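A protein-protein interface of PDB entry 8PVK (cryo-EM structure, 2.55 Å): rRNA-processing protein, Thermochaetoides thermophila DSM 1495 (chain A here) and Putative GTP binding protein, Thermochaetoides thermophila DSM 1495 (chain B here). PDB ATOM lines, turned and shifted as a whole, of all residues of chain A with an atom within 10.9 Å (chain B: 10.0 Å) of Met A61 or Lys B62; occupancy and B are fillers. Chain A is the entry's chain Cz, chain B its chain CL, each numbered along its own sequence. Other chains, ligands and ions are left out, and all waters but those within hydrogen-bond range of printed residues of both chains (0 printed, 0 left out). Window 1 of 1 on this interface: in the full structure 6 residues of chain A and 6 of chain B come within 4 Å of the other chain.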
ATOM      1  N   LYS A  53      11.963 -15.749 -22.844  1.00  0.00           N
ATOM      2  CA  LYS A  53      12.456 -15.266 -21.555  1.00  0.00           C
ATOM      3  C   LYS A  53      11.780 -13.955 -21.158  1.00  0.00           C
ATOM      4  O   LYS A  53      11.396 -13.770 -19.992  1.00  0.00           O
ATOM      5  CB  LYS A  53      13.975 -15.106 -21.623  1.00  0.00           C
ATOM      6  CG  LYS A  53      14.593 -14.243 -20.541  1.00  0.00           C
ATOM      7  CD  LYS A  53      16.092 -14.108 -20.767  1.00  0.00           C
ATOM      8  CE  LYS A  53      16.739 -13.221 -19.720  1.00  0.00           C
ATOM      9  NZ  LYS A  53      18.205 -13.089 -19.937  1.00  0.00           N
ATOM     10  N   LYS A  54      11.599 -13.048 -22.122  1.00  0.00           N
ATOM     11  CA  LYS A  54      10.897 -11.798 -21.851  1.00  0.00           C
ATOM     12  C   LYS A  54       9.427 -12.030 -21.521  1.00  0.00           C
ATOM     13  O   LYS A  54       8.866 -11.307 -20.692  1.00  0.00           O
ATOM     14  CB  LYS A  54      11.030 -10.849 -23.041  1.00  0.00           C
ATOM     15  CG  LYS A  54      12.421 -10.262 -23.216  1.00  0.00           C
ATOM     16  CD  LYS A  54      12.934  -9.645 -21.926  1.00  0.00           C
ATOM     17  CE  LYS A  54      14.381  -9.201 -22.064  1.00  0.00           C
ATOM     18  NZ  LYS A  54      14.900  -8.594 -20.808  1.00  0.00           N
ATOM     19  N   ARG A  55       8.793 -13.023 -22.155  1.00  0.00           N
ATOM     20  CA  ARG A  55       7.419 -13.384 -21.817  1.00  0.00           C
ATOM     21  C   ARG A  55       7.311 -13.834 -20.367  1.00  0.00           C
ATOM     22  O   ARG A  55       6.403 -13.411 -19.638  1.00  0.00           O
ATOM     23  CB  ARG A  55       6.922 -14.495 -22.743  1.00  0.00           C
ATOM     24  CG  ARG A  55       6.454 -14.051 -24.112  1.00  0.00           C
ATOM     25  CD  ARG A  55       6.174 -15.263 -24.987  1.00  0.00           C
ATOM     26  NE  ARG A  55       5.120 -16.107 -24.435  1.00  0.00           N
ATOM     27  CZ  ARG A  55       4.677 -17.219 -25.001  1.00  0.00           C
ATOM     28  NH1 ARG A  55       5.186 -17.668 -26.137  1.00  0.00           N
ATOM     29  NH2 ARG A  55       3.699 -17.902 -24.413  1.00  0.00           N
ATOM     30  N   GLN A  56       8.243 -14.691 -19.932  1.00  0.00           N
ATOM     31  CA  GLN A  56       8.231 -15.162 -18.547  1.00  0.00           C
ATOM     32  C   GLN A  56       8.446 -14.014 -17.564  1.00  0.00           C
ATOM     33  O   GLN A  56       7.734 -13.906 -16.552  1.00  0.00           O
ATOM     34  CB  GLN A  56       9.296 -16.240 -18.349  1.00  0.00           C
ATOM     35  CG  GLN A  56       9.073 -17.499 -19.168  1.00  0.00           C
ATOM     36  CD  GLN A  56      10.295 -18.396 -19.199  1.00  0.00           C
ATOM     37  OE1 GLN A  56      11.335 -18.064 -18.632  1.00  0.00           O
ATOM     38  NE2 GLN A  56      10.174 -19.539 -19.862  1.00  0.00           N
ATOM     39  N   GLU A  57       9.414 -13.136 -17.858  1.00  0.00           N
ATOM     40  CA  GLU A  57       9.693 -12.011 -16.968  1.00  0.00           C
ATOM     41  C   GLU A  57       8.518 -11.041 -16.900  1.00  0.00           C
ATOM     42  O   GLU A  57       8.176 -10.549 -15.815  1.00  0.00           O
ATOM     43  CB  GLU A  57      10.962 -11.288 -17.416  1.00  0.00           C
ATOM     44  CG  GLU A  57      12.225 -12.117 -17.268  1.00  0.00           C
ATOM     45  CD  GLU A  57      13.452 -11.407 -17.796  1.00  0.00           C
ATOM     46  OE1 GLU A  57      13.302 -10.323 -18.398  1.00  0.00           O
ATOM     47  OE2 GLU A  57      14.569 -11.929 -17.603  1.00  0.00           O
ATOM     48  N   GLN A  58       7.877 -10.764 -18.040  1.00  0.00           N
ATOM     49  CA  GLN A  58       6.734  -9.858 -18.049  1.00  0.00           C
ATOM     50  C   GLN A  58       5.540 -10.459 -17.320  1.00  0.00           C
ATOM     51  O   GLN A  58       4.803  -9.738 -16.639  1.00  0.00           O
ATOM     52  CB  GLN A  58       6.360  -9.495 -19.487  1.00  0.00           C
ATOM     53  CG  GLN A  58       7.288  -8.479 -20.146  1.00  0.00           C
ATOM     54  CD  GLN A  58       7.289  -7.131 -19.448  1.00  0.00           C
ATOM     55  OE1 GLN A  58       6.418  -6.295 -19.688  1.00  0.00           O
ATOM     56  NE2 GLN A  58       8.279  -6.908 -18.589  1.00  0.00           N
ATOM     57  N   ALA A  59       5.334 -11.775 -17.447  1.00  0.00           N
ATOM     58  CA  ALA A  59       4.253 -12.428 -16.711  1.00  0.00           C
ATOM     59  C   ALA A  59       4.476 -12.346 -15.205  1.00  0.00           C
ATOM     60  O   ALA A  59       3.539 -12.055 -14.446  1.00  0.00           O
ATOM     61  CB  ALA A  59       4.121 -13.883 -17.156  1.00  0.00           C
ATOM     62  N   ALA A  60       5.716 -12.581 -14.756  1.00  0.00           N
ATOM     63  CA  ALA A  60       6.021 -12.464 -13.331  1.00  0.00           C
ATOM     64  C   ALA A  60       5.839 -11.032 -12.836  1.00  0.00           C
ATOM     65  O   ALA A  60       5.316 -10.805 -11.734  1.00  0.00           O
ATOM     66  CB  ALA A  60       7.443 -12.950 -13.057  1.00  0.00           C
ATOM     67  N   MET A  61       6.259 -10.054 -13.647  1.00  0.00           N
ATOM     68  CA  MET A  61       6.096  -8.648 -13.289  1.00  0.00           C
ATOM     69  C   MET A  61       4.623  -8.272 -13.163  1.00  0.00           C
ATOM     70  O   MET A  61       4.232  -7.580 -12.212  1.00  0.00           O
ATOM     71  CB  MET A  61       6.813  -7.779 -14.329  1.00  0.00           C
ATOM     72  CG  MET A  61       6.814  -6.266 -14.101  1.00  0.00           C
ATOM     73  SD  MET A  61       5.326  -5.392 -14.636  1.00  0.00           S
ATOM     74  CE  MET A  61       5.518  -5.469 -16.414  1.00  0.00           C
ATOM     75  N   LYS A  62       3.792  -8.718 -14.112  1.00  0.00           N
ATOM     76  CA  LYS A  62       2.365  -8.414 -14.054  1.00  0.00           C
ATOM     77  C   LYS A  62       1.704  -9.074 -12.851  1.00  0.00           C
ATOM     78  O   LYS A  62       0.823  -8.477 -12.217  1.00  0.00           O
ATOM     79  CB  LYS A  62       1.675  -8.850 -15.347  1.00  0.00           C
ATOM     80  CG  LYS A  62       2.063  -8.038 -16.574  1.00  0.00           C
ATOM     81  CD  LYS A  62       1.872  -6.549 -16.350  1.00  0.00           C
ATOM     82  CE  LYS A  62       0.402  -6.180 -16.319  1.00  0.00           C
ATOM     83  NZ  LYS A  62       0.205  -4.714 -16.156  1.00  0.00           N
ATOM     84  N   ALA A  63       2.117 -10.305 -12.521  1.00  0.00           N
ATOM     85  CA  ALA A  63       1.572 -10.977 -11.344  1.00  0.00           C
ATOM     86  C   ALA A  63       1.913 -10.225 -10.061  1.00  0.00           C
ATOM     87  O   ALA A  63       1.038 -10.005  -9.211  1.00  0.00           O
ATOM     88  CB  ALA A  63       2.089 -12.414 -11.277  1.00  0.00           C
ATOM     89  N   LYS A  64       3.172  -9.797  -9.915  1.00  0.00           N
ATOM     90  CA  LYS A  64       3.553  -9.048  -8.718  1.00  0.00           C
ATOM     91  C   LYS A  64       2.822  -7.708  -8.645  1.00  0.00           C
ATOM     92  O   LYS A  64       2.374  -7.292  -7.565  1.00  0.00           O
ATOM     93  CB  LYS A  64       5.065  -8.834  -8.677  1.00  0.00           C
ATOM     94  CG  LYS A  64       5.517  -8.093  -7.433  1.00  0.00           C
ATOM     95  CD  LYS A  64       6.962  -7.652  -7.500  1.00  0.00           C
ATOM     96  CE  LYS A  64       7.334  -6.908  -6.229  1.00  0.00           C
ATOM     97  NZ  LYS A  64       8.694  -6.320  -6.304  1.00  0.00           N
ATOM     98  N   GLU A  65       2.672  -7.033  -9.791  1.00  0.00           N
ATOM     99  CA  GLU A  65       1.985  -5.745  -9.818  1.00  0.00           C
ATOM    100  C   GLU A  65       0.515  -5.883  -9.436  1.00  0.00           C
ATOM    101  O   GLU A  65      -0.019  -5.048  -8.694  1.00  0.00           O
ATOM    102  CB  GLU A  65       2.122  -5.107 -11.200  1.00  0.00           C
ATOM    103  CG  GLU A  65       1.550  -3.701 -11.295  1.00  0.00           C
ATOM    104  CD  GLU A  65       1.242  -3.294 -12.723  1.00  0.00           C
ATOM    105  OE1 GLU A  65       1.226  -4.179 -13.603  1.00  0.00           O
ATOM    106  OE2 GLU A  65       1.015  -2.090 -12.965  1.00  0.00           O
ATOM    107  N   ARG A  66      -0.159  -6.933  -9.920  1.00  0.00           N
ATOM    108  CA  ARG A  66      -1.566  -7.082  -9.565  1.00  0.00           C
ATOM    109  C   ARG A  66      -1.741  -7.515  -8.113  1.00  0.00           C
ATOM    110  O   ARG A  66      -2.727  -7.122  -7.478  1.00  0.00           O
ATOM    111  CB  ARG A  66      -2.283  -8.043 -10.520  1.00  0.00           C
ATOM    112  CG  ARG A  66      -1.866  -9.494 -10.451  1.00  0.00           C
ATOM    113  CD  ARG A  66      -2.577 -10.310 -11.516  1.00  0.00           C
ATOM    114  NE  ARG A  66      -2.135  -9.957 -12.860  1.00  0.00           N
ATOM    115  CZ  ARG A  66      -2.694 -10.409 -13.974  1.00  0.00           C
ATOM    116  NH1 ARG A  66      -3.723 -11.239 -13.943  1.00  0.00           N
ATOM    117  NH2 ARG A  66      -2.209 -10.018 -15.149  1.00  0.00           N
ATOM    118  N   GLU A  67      -0.792  -8.281  -7.551  1.00  0.00           N
ATOM    119  CA  GLU A  67      -0.852  -8.561  -6.113  1.00  0.00           C
ATOM    120  C   GLU A  67      -0.699  -7.286  -5.285  1.00  0.00           C
ATOM    121  O   GLU A  67      -1.428  -7.081  -4.301  1.00  0.00           O
ATOM    122  CB  GLU A  67       0.215  -9.582  -5.709  1.00  0.00           C
ATOM    123  CG  GLU A  67       0.084 -10.971  -6.335  1.00  0.00           C
ATOM    124  CD  GLU A  67      -1.268 -11.628  -6.100  1.00  0.00           C
ATOM    125  OE1 GLU A  67      -1.866 -11.419  -5.023  1.00  0.00           O
ATOM    126  OE2 GLU A  67      -1.731 -12.363  -6.997  1.00  0.00           O
ATOM    127  N   MET A  68       0.239  -6.415  -5.674  1.00  0.00           N
ATOM    128  CA  MET A  68       0.440  -5.156  -4.956  1.00  0.00           C
ATOM    129  C   MET A  68      -0.789  -4.251  -5.063  1.00  0.00           C
ATOM    130  O   MET A  68      -1.203  -3.621  -4.075  1.00  0.00           O
ATOM    131  CB  MET A  68       1.692  -4.469  -5.503  1.00  0.00           C
ATOM    132  CG  MET A  68       2.983  -5.198  -5.133  1.00  0.00           C
ATOM    133  SD  MET A  68       4.493  -4.488  -5.824  1.00  0.00           S
ATOM    134  CE  MET A  68       4.472  -2.838  -5.144  1.00  0.00           C
ATOM    135  N   LYS A  69      -1.403  -4.203  -6.251  1.00  0.00           N
ATOM    136  CA  LYS A  69      -2.618  -3.415  -6.440  1.00  0.00           C
ATOM    137  C   LYS A  69      -3.779  -3.963  -5.617  1.00  0.00           C
ATOM    138  O   LYS A  69      -4.562  -3.189  -5.052  1.00  0.00           O
ATOM    139  CB  LYS A  69      -2.986  -3.374  -7.923  1.00  0.00           C
ATOM    140  CG  LYS A  69      -2.132  -2.426  -8.744  1.00  0.00           C
ATOM    141  CD  LYS A  69      -2.573  -2.409 -10.196  1.00  0.00           C
ATOM    142  CE  LYS A  69      -1.947  -1.249 -10.945  1.00  0.00           C
ATOM    143  NZ  LYS A  69      -2.335  -1.257 -12.380  1.00  0.00           N
ATOM    144  N   GLU A  70      -3.908  -5.293  -5.538  1.00  0.00           N
ATOM    145  CA  GLU A  70      -4.968  -5.894  -4.734  1.00  0.00           C
ATOM    146  C   GLU A  70      -4.782  -5.597  -3.251  1.00  0.00           C
ATOM    147  O   GLU A  70      -5.760  -5.333  -2.538  1.00  0.00           O
ATOM    148  CB  GLU A  70      -5.020  -7.403  -4.973  1.00  0.00           C
ATOM    149  CG  GLU A  70      -5.709  -7.807  -6.264  1.00  0.00           C
ATOM    150  CD  GLU A  70      -5.329  -9.204  -6.710  1.00  0.00           C
ATOM    151  OE1 GLU A  70      -4.583  -9.883  -5.973  1.00  0.00           O
ATOM    152  OE2 GLU A  70      -5.776  -9.626  -7.796  1.00  0.00           O
ATOM    153  N   PRO B  53      -1.408   7.150 -13.415  1.00  0.00           N
ATOM    154  CA  PRO B  53      -1.393   6.049 -14.388  1.00  0.00           C
ATOM    155  C   PRO B  53      -0.426   4.929 -14.031  1.00  0.00           C
ATOM    156  O   PRO B  53      -0.681   3.766 -14.354  1.00  0.00           O
ATOM    157  CB  PRO B  53      -0.991   6.742 -15.699  1.00  0.00           C
ATOM    158  CG  PRO B  53      -1.109   8.214 -15.438  1.00  0.00           C
ATOM    159  CD  PRO B  53      -0.859   8.390 -13.984  1.00  0.00           C
ATOM    160  N   GLY B  54       0.680   5.257 -13.375  1.00  0.00           N
ATOM    161  CA  GLY B  54       1.614   4.251 -12.909  1.00  0.00           C
ATOM    162  C   GLY B  54       2.865   4.137 -13.759  1.00  0.00           C
ATOM    163  O   GLY B  54       3.280   5.066 -14.456  1.00  0.00           O
ATOM    164  N   ILE B  55       3.474   2.963 -13.686  1.00  0.00           N
ATOM    165  CA  ILE B  55       4.720   2.661 -14.391  1.00  0.00           C
ATOM    166  C   ILE B  55       4.375   1.917 -15.677  1.00  0.00           C
ATOM    167  O   ILE B  55       3.557   0.987 -15.634  1.00  0.00           O
ATOM    168  CB  ILE B  55       5.673   1.825 -13.515  1.00  0.00           C
ATOM    169  CG1 ILE B  55       5.677   2.347 -12.078  1.00  0.00           C
ATOM    170  CG2 ILE B  55       7.082   1.832 -14.084  1.00  0.00           C
ATOM    171  CD1 ILE B  55       6.267   1.376 -11.080  1.00  0.00           C
ATOM    172  N   PRO B  56       4.943   2.298 -16.821  1.00  0.00           N
ATOM    173  CA  PRO B  56       4.655   1.577 -18.066  1.00  0.00           C
ATOM    174  C   PRO B  56       5.218   0.165 -18.054  1.00  0.00           C
ATOM    175  O   PRO B  56       6.239  -0.121 -17.424  1.00  0.00           O
ATOM    176  CB  PRO B  56       5.338   2.434 -19.141  1.00  0.00           C
ATOM    177  CG  PRO B  56       5.529   3.768 -18.511  1.00  0.00           C
ATOM    178  CD  PRO B  56       5.760   3.496 -17.062  1.00  0.00           C
ATOM    179  N   ASN B  57       4.536  -0.722 -18.783  1.00  0.00           N
ATOM    180  CA  ASN B  57       4.930  -2.127 -18.802  1.00  0.00           C
ATOM    181  C   ASN B  57       6.182  -2.359 -19.636  1.00  0.00           C
ATOM    182  O   ASN B  57       6.947  -3.288 -19.352  1.00  0.00           O
ATOM    183  CB  ASN B  57       3.780  -2.985 -19.325  1.00  0.00           C
ATOM    184  CG  ASN B  57       2.565  -2.942 -18.424  1.00  0.00           C
ATOM    185  OD1 ASN B  57       2.672  -2.664 -17.231  1.00  0.00           O
ATOM    186  ND2 ASN B  57       1.398  -3.217 -18.993  1.00  0.00           N
ATOM    187  N   LEU B  58       6.413  -1.538 -20.660  1.00  0.00           N
ATOM    188  CA  LEU B  58       7.582  -1.720 -21.511  1.00  0.00           C
ATOM    189  C   LEU B  58       8.849  -1.121 -20.919  1.00  0.00           C
ATOM    190  O   LEU B  58       9.923  -1.285 -21.510  1.00  0.00           O
ATOM    191  CB  LEU B  58       7.329  -1.128 -22.899  1.00  0.00           C
ATOM    192  CG  LEU B  58       6.247  -1.836 -23.715  1.00  0.00           C
ATOM    193  CD1 LEU B  58       5.978  -1.097 -25.010  1.00  0.00           C
ATOM    194  CD2 LEU B  58       6.651  -3.274 -23.994  1.00  0.00           C
ATOM    195  N   PHE B  59       8.754  -0.429 -19.791  1.00  0.00           N
ATOM    196  CA  PHE B  59       9.939  -0.012 -19.061  1.00  0.00           C
ATOM    197  C   PHE B  59      10.646  -1.254 -18.528  1.00  0.00           C
ATOM    198  O   PHE B  59      10.023  -2.044 -17.802  1.00  0.00           O
ATOM    199  CB  PHE B  59       9.558   0.926 -17.920  1.00  0.00           C
ATOM    200  CG  PHE B  59      10.732   1.474 -17.166  1.00  0.00           C
ATOM    201  CD1 PHE B  59      11.677   2.258 -17.807  1.00  0.00           C
ATOM    202  CD2 PHE B  59      10.893   1.205 -15.818  1.00  0.00           C
ATOM    203  CE1 PHE B  59      12.758   2.766 -17.116  1.00  0.00           C
ATOM    204  CE2 PHE B  59      11.972   1.709 -15.122  1.00  0.00           C
ATOM    205  CZ  PHE B  59      12.907   2.488 -15.774  1.00  0.00           C
ATOM    206  N   PRO B  60      11.922  -1.474 -18.863  1.00  0.00           N
ATOM    207  CA  PRO B  60      12.545  -2.777 -18.574  1.00  0.00           C
ATOM    208  C   PRO B  60      12.849  -3.017 -17.105  1.00  0.00           C
ATOM    209  O   PRO B  60      13.114  -4.165 -16.731  1.00  0.00           O
ATOM    210  CB  PRO B  60      13.839  -2.741 -19.404  1.00  0.00           C
ATOM    211  CG  PRO B  60      13.668  -1.599 -20.364  1.00  0.00           C
ATOM    212  CD  PRO B  60      12.804  -0.609 -19.660  1.00  0.00           C
ATOM    213  N   TYR B  61      12.820  -1.985 -16.264  1.00  0.00           N
ATOM    214  CA  TYR B  61      13.192  -2.106 -14.860  1.00  0.00           C
ATOM    215  C   TYR B  61      12.009  -1.819 -13.940  1.00  0.00           C
ATOM    216  O   TYR B  61      12.183  -1.345 -12.813  1.00  0.00           O
ATOM    217  CB  TYR B  61      14.371  -1.187 -14.544  1.00  0.00           C
ATOM    218  CG  TYR B  61      15.541  -1.371 -15.486  1.00  0.00           C
ATOM    219  CD1 TYR B  61      15.990  -2.642 -15.830  1.00  0.00           C
ATOM    220  CD2 TYR B  61      16.184  -0.277 -16.049  1.00  0.00           C
ATOM    221  CE1 TYR B  61      17.053  -2.816 -16.698  1.00  0.00           C
ATOM    222  CE2 TYR B  61      17.249  -0.442 -16.918  1.00  0.00           C
ATOM    223  CZ  TYR B  61      17.678  -1.715 -17.237  1.00  0.00           C
ATOM    224  OH  TYR B  61      18.736  -1.887 -18.100  1.00  0.00           O
ATOM    225  N   LYS B  62      10.796  -2.111 -14.420  1.00  0.00           N
ATOM    226  CA  LYS B  62       9.605  -1.977 -13.589  1.00  0.00           C
ATOM    227  C   LYS B  62       9.632  -2.960 -12.425  1.00  0.00           C
ATOM    228  O   LYS B  62       9.169  -2.638 -11.325  1.00  0.00           O
ATOM    229  CB  LYS B  62       8.352  -2.178 -14.441  1.00  0.00           C
ATOM    230  CG  LYS B  62       7.041  -1.955 -13.706  1.00  0.00           C
ATOM    231  CD  LYS B  62       5.885  -1.855 -14.678  1.00  0.00           C
ATOM    232  CE  LYS B  62       4.562  -1.697 -13.958  1.00  0.00           C
ATOM    233  NZ  LYS B  62       3.426  -1.612 -14.914  1.00  0.00           N
ATOM    234  N   GLU B  63      10.174  -4.160 -12.649  1.00  0.00           N
ATOM    235  CA  GLU B  63      10.326  -5.126 -11.566  1.00  0.00           C
ATOM    236  C   GLU B  63      11.259  -4.611 -10.475  1.00  0.00           C
ATOM    237  O   GLU B  63      10.942  -4.733  -9.288  1.00  0.00           O
ATOM    238  CB  GLU B  63      10.837  -6.458 -12.119  1.00  0.00           C
ATOM    239  CG  GLU B  63      10.996  -7.564 -11.081  1.00  0.00           C
ATOM    240  CD  GLU B  63       9.680  -8.007 -10.461  1.00  0.00           C
ATOM    241  OE1 GLU B  63       8.623  -7.860 -11.111  1.00  0.00           O
ATOM    242  OE2 GLU B  63       9.706  -8.505  -9.316  1.00  0.00           O
ATOM    243  N   ARG B  64      12.391  -4.011 -10.855  1.00  0.00           N
ATOM    244  CA  ARG B  64      13.297  -3.442  -9.860  1.00  0.00           C
ATOM    245  C   ARG B  64      12.685  -2.224  -9.176  1.00  0.00           C
ATOM    246  O   ARG B  64      12.952  -1.974  -7.994  1.00  0.00           O
ATOM    247  CB  ARG B  64      14.638  -3.090 -10.503  1.00  0.00           C
ATOM    248  CG  ARG B  64      15.702  -4.158 -10.308  1.00  0.00           C
ATOM    249  CD  ARG B  64      17.052  -3.726 -10.852  1.00  0.00           C
ATOM    250  NE  ARG B  64      17.296  -4.257 -12.188  1.00  0.00           N
ATOM    251  CZ  ARG B  64      18.187  -3.768 -13.039  1.00  0.00           C
ATOM    252  NH1 ARG B  64      18.905  -2.696 -12.748  1.00  0.00           N
ATOM    253  NH2 ARG B  64      18.371  -4.377 -14.205  1.00  0.00           N
ATOM    254  N   LEU B  65      11.855  -1.461  -9.896  1.00  0.00           N
ATOM    255  CA  LEU B  65      11.130  -0.364  -9.258  1.00  0.00           C
ATOM    256  C   LEU B  65      10.152  -0.880  -8.209  1.00  0.00           C
ATOM    257  O   LEU B  65      10.019  -0.292  -7.128  1.00  0.00           O
ATOM    258  CB  LEU B  65      10.398   0.466 -10.311  1.00  0.00           C
ATOM    259  CG  LEU B  65      11.172   1.659 -10.869  1.00  0.00           C
ATOM    260  CD1 LEU B  65      10.317   2.425 -11.858  1.00  0.00           C
ATOM    261  CD2 LEU B  65      11.628   2.562  -9.736  1.00  0.00           C
ATOM    262  N   LEU B  66       9.461  -1.983  -8.509  1.00  0.00           N
ATOM    263  CA  LEU B  66       8.546  -2.575  -7.537  1.00  0.00           C
ATOM    264  C   LEU B  66       9.304  -3.148  -6.341  1.00  0.00           C
ATOM    265  O   LEU B  66       8.824  -3.071  -5.201  1.00  0.00           O
ATOM    266  CB  LEU B  66       7.698  -3.654  -8.210  1.00  0.00           C
ATOM    267  CG  LEU B  66       6.681  -3.160  -9.243  1.00  0.00           C
ATOM    268  CD1 LEU B  66       5.994  -4.331  -9.928  1.00  0.00           C
ATOM    269  CD2 LEU B  66       5.662  -2.213  -8.631  1.00  0.00           C
ATOM    270  N   GLN B  67      10.487  -3.724  -6.586  1.00  0.00           N
ATOM    271  CA  GLN B  67      11.352  -4.166  -5.492  1.00  0.00           C
ATOM    272  C   GLN B  67      11.755  -3.000  -4.599  1.00  0.00           C
ATOM    273  O   GLN B  67      11.746  -3.118  -3.366  1.00  0.00           O
ATOM    274  CB  GLN B  67      12.603  -4.853  -6.042  1.00  0.00           C
ATOM    275  CG  GLN B  67      12.366  -6.153  -6.785  1.00  0.00           C
ATOM    276  CD  GLN B  67      11.768  -7.220  -5.899  1.00  0.00           C
ATOM    277  OE1 GLN B  67      10.604  -7.586  -6.042  1.00  0.00           O
ATOM    278  NE2 GLN B  67      12.561  -7.718  -4.959  1.00  0.00           N
ATOM    279  N   GLN B  68      12.111  -1.868  -5.208  1.00  0.00           N
ATOM    280  CA  GLN B  68      12.478  -0.682  -4.442  1.00  0.00           C
ATOM    281  C   GLN B  68      11.296  -0.152  -3.639  1.00  0.00           C
ATOM    282  O   GLN B  68      11.468   0.310  -2.507  1.00  0.00           O
ATOM    283  CB  GLN B  68      13.015   0.392  -5.383  1.00  0.00           C
ATOM    284  CG  GLN B  68      14.486   0.230  -5.711  1.00  0.00           C
ATOM    285  CD  GLN B  68      15.059   1.436  -6.418  1.00  0.00           C
ATOM    286  OE1 GLN B  68      14.480   2.522  -6.388  1.00  0.00           O
ATOM    287  NE2 GLN B  68      16.203   1.253  -7.065  1.00  0.00           N
ATOM    288  N   ILE B  69      10.092  -0.207  -4.214  1.00  0.00           N
ATOM    289  CA  ILE B  69       8.903   0.266  -3.509  1.00  0.00           C
ATOM    290  C   ILE B  69       8.593  -0.625  -2.305  1.00  0.00           C
ATOM    291  O   ILE B  69       8.293  -0.123  -1.212  1.00  0.00           O
ATOM    292  CB  ILE B  69       7.717   0.366  -4.486  1.00  0.00           C
ATOM    293  CG1 ILE B  69       7.911   1.567  -5.414  1.00  0.00           C
ATOM    294  CG2 ILE B  69       6.402   0.521  -3.744  1.00  0.00           C
ATOM    295  CD1 ILE B  69       6.985   1.581  -6.606  1.00  0.00           C
ATOM    296  N   GLU B  70       8.686  -1.952  -2.479  1.00  0.00           N
ATOM    297  CA  GLU B  70       8.537  -2.871  -1.346  1.00  0.00           C
ATOM    298  C   GLU B  70       9.574  -2.610  -0.263  1.00  0.00           C
ATOM    299  O   GLU B  70       9.240  -2.562   0.928  1.00  0.00           O
ATOM    300  CB  GLU B  70       8.633  -4.327  -1.809  1.00  0.00           C
ATOM    301  CG  GLU B  70       7.508  -4.818  -2.694  1.00  0.00           C
ATOM    302  CD  GLU B  70       6.182  -4.880  -1.949  1.00  0.00           C
ATOM    303  OE1 GLU B  70       6.201  -5.136  -0.725  1.00  0.00           O
ATOM    304  OE2 GLU B  70       5.121  -4.709  -2.582  1.00  0.00           O
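The side-chain carboxylate (OE2) of Glu B63 lies within salt-bridge range of the side-chain amino group (NZ) of Lys A64, 3.9 Å away.
OE2 of Glu B70 lies close to SD of Met A68, at 3.3 Å.
OE1 of Gln A58 sits close to O of Asn B57, at 3.1 Å.
OE2 of Glu A65 lies within salt-bridge range of NZ of Lys B62.
O of Leu B66 lies close to NZ of Lys A64 (3.4 Å).
NZ of Lys A64 sits close to OE1 of Gln B67 (2.3 Å).
OD1 of Asn B57 sits at hydrogen-bond distance from NZ of Lys A62, 3.4 Å away.
O of Ile B55 is in hydrogen-bond range of NZ of Lys B62, at 2.7 Å.
O of Lys A62 sits at hydrogen-bond distance from NE of Arg A66 (3.4 Å).
The side-chain carboxylate (OE1) of Glu A65 is in salt-bridge range of the side-chain amino group (NZ) of Lys A62 (2.8 Å).
The side-chain carboxylate (OE2) of Glu A65 lies within salt-bridge range of the side-chain amino group (NZ) of Lys A69 (3.5 Å).
The side-chain amino group (NZ) of Lys B62 lies within hydrogen-bond range of the side-chain amide oxygen (OD1) of Asn B57.
Met A61 touches Asn B57.
Lys B62 touches Met A61.
Met A61 touches Glu B63 (CA to OE1, 3.4 Å).
Met A68 touches Leu B66 (CE to CD2, 3.7 Å).
Arg A55 touches none of the printed residues of chain B.
Gln A58 touches just one residue of chain B: Asn B57.
No residue of chain B comes within 4 Å of Ala A59.
No residue of chain B comes within 4 Å of Ala A60.
Of chain B, only Asn B57 (3.9 Å), Lys B62 (3.6 Å) and Glu B63 (3.4 Å) come within 4 Å of Met A61.
Printed residues of chain B within 4 Å of Lys A64: Glu B63 (3.4 Å), Leu B66 (3.2 Å) and Gln B67 (2.3 Å).
Of the printed residues of chain B, Glu A65 touches Lys B62.
Printed residues of chain B within 4 Å of Met A68: Leu B66 and Glu B70.
Lys A69 touches none of the printed residues of chain B.
No residue of chain A comes within 4 Å of Ile B55.
Of chain A, only Met A61 (3.6 Å) and Glu A65 (3.1 Å) come within 4 Å of Lys B62.
No residue of chain A comes within 4 Å of Leu B65.
Of the printed residues of chain A, Gln B67 touches Lys A64.
Of the printed residues of chain A, Glu B70 touches Met A68.
Of the 18 printed residues of chain B, 6 touch a printed residue of chain A.
Printed residues of chain B that touch a printed residue of chain A: Asn B57, Lys B62, Glu B63, Leu B66, Gln B67 and Glu B70.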
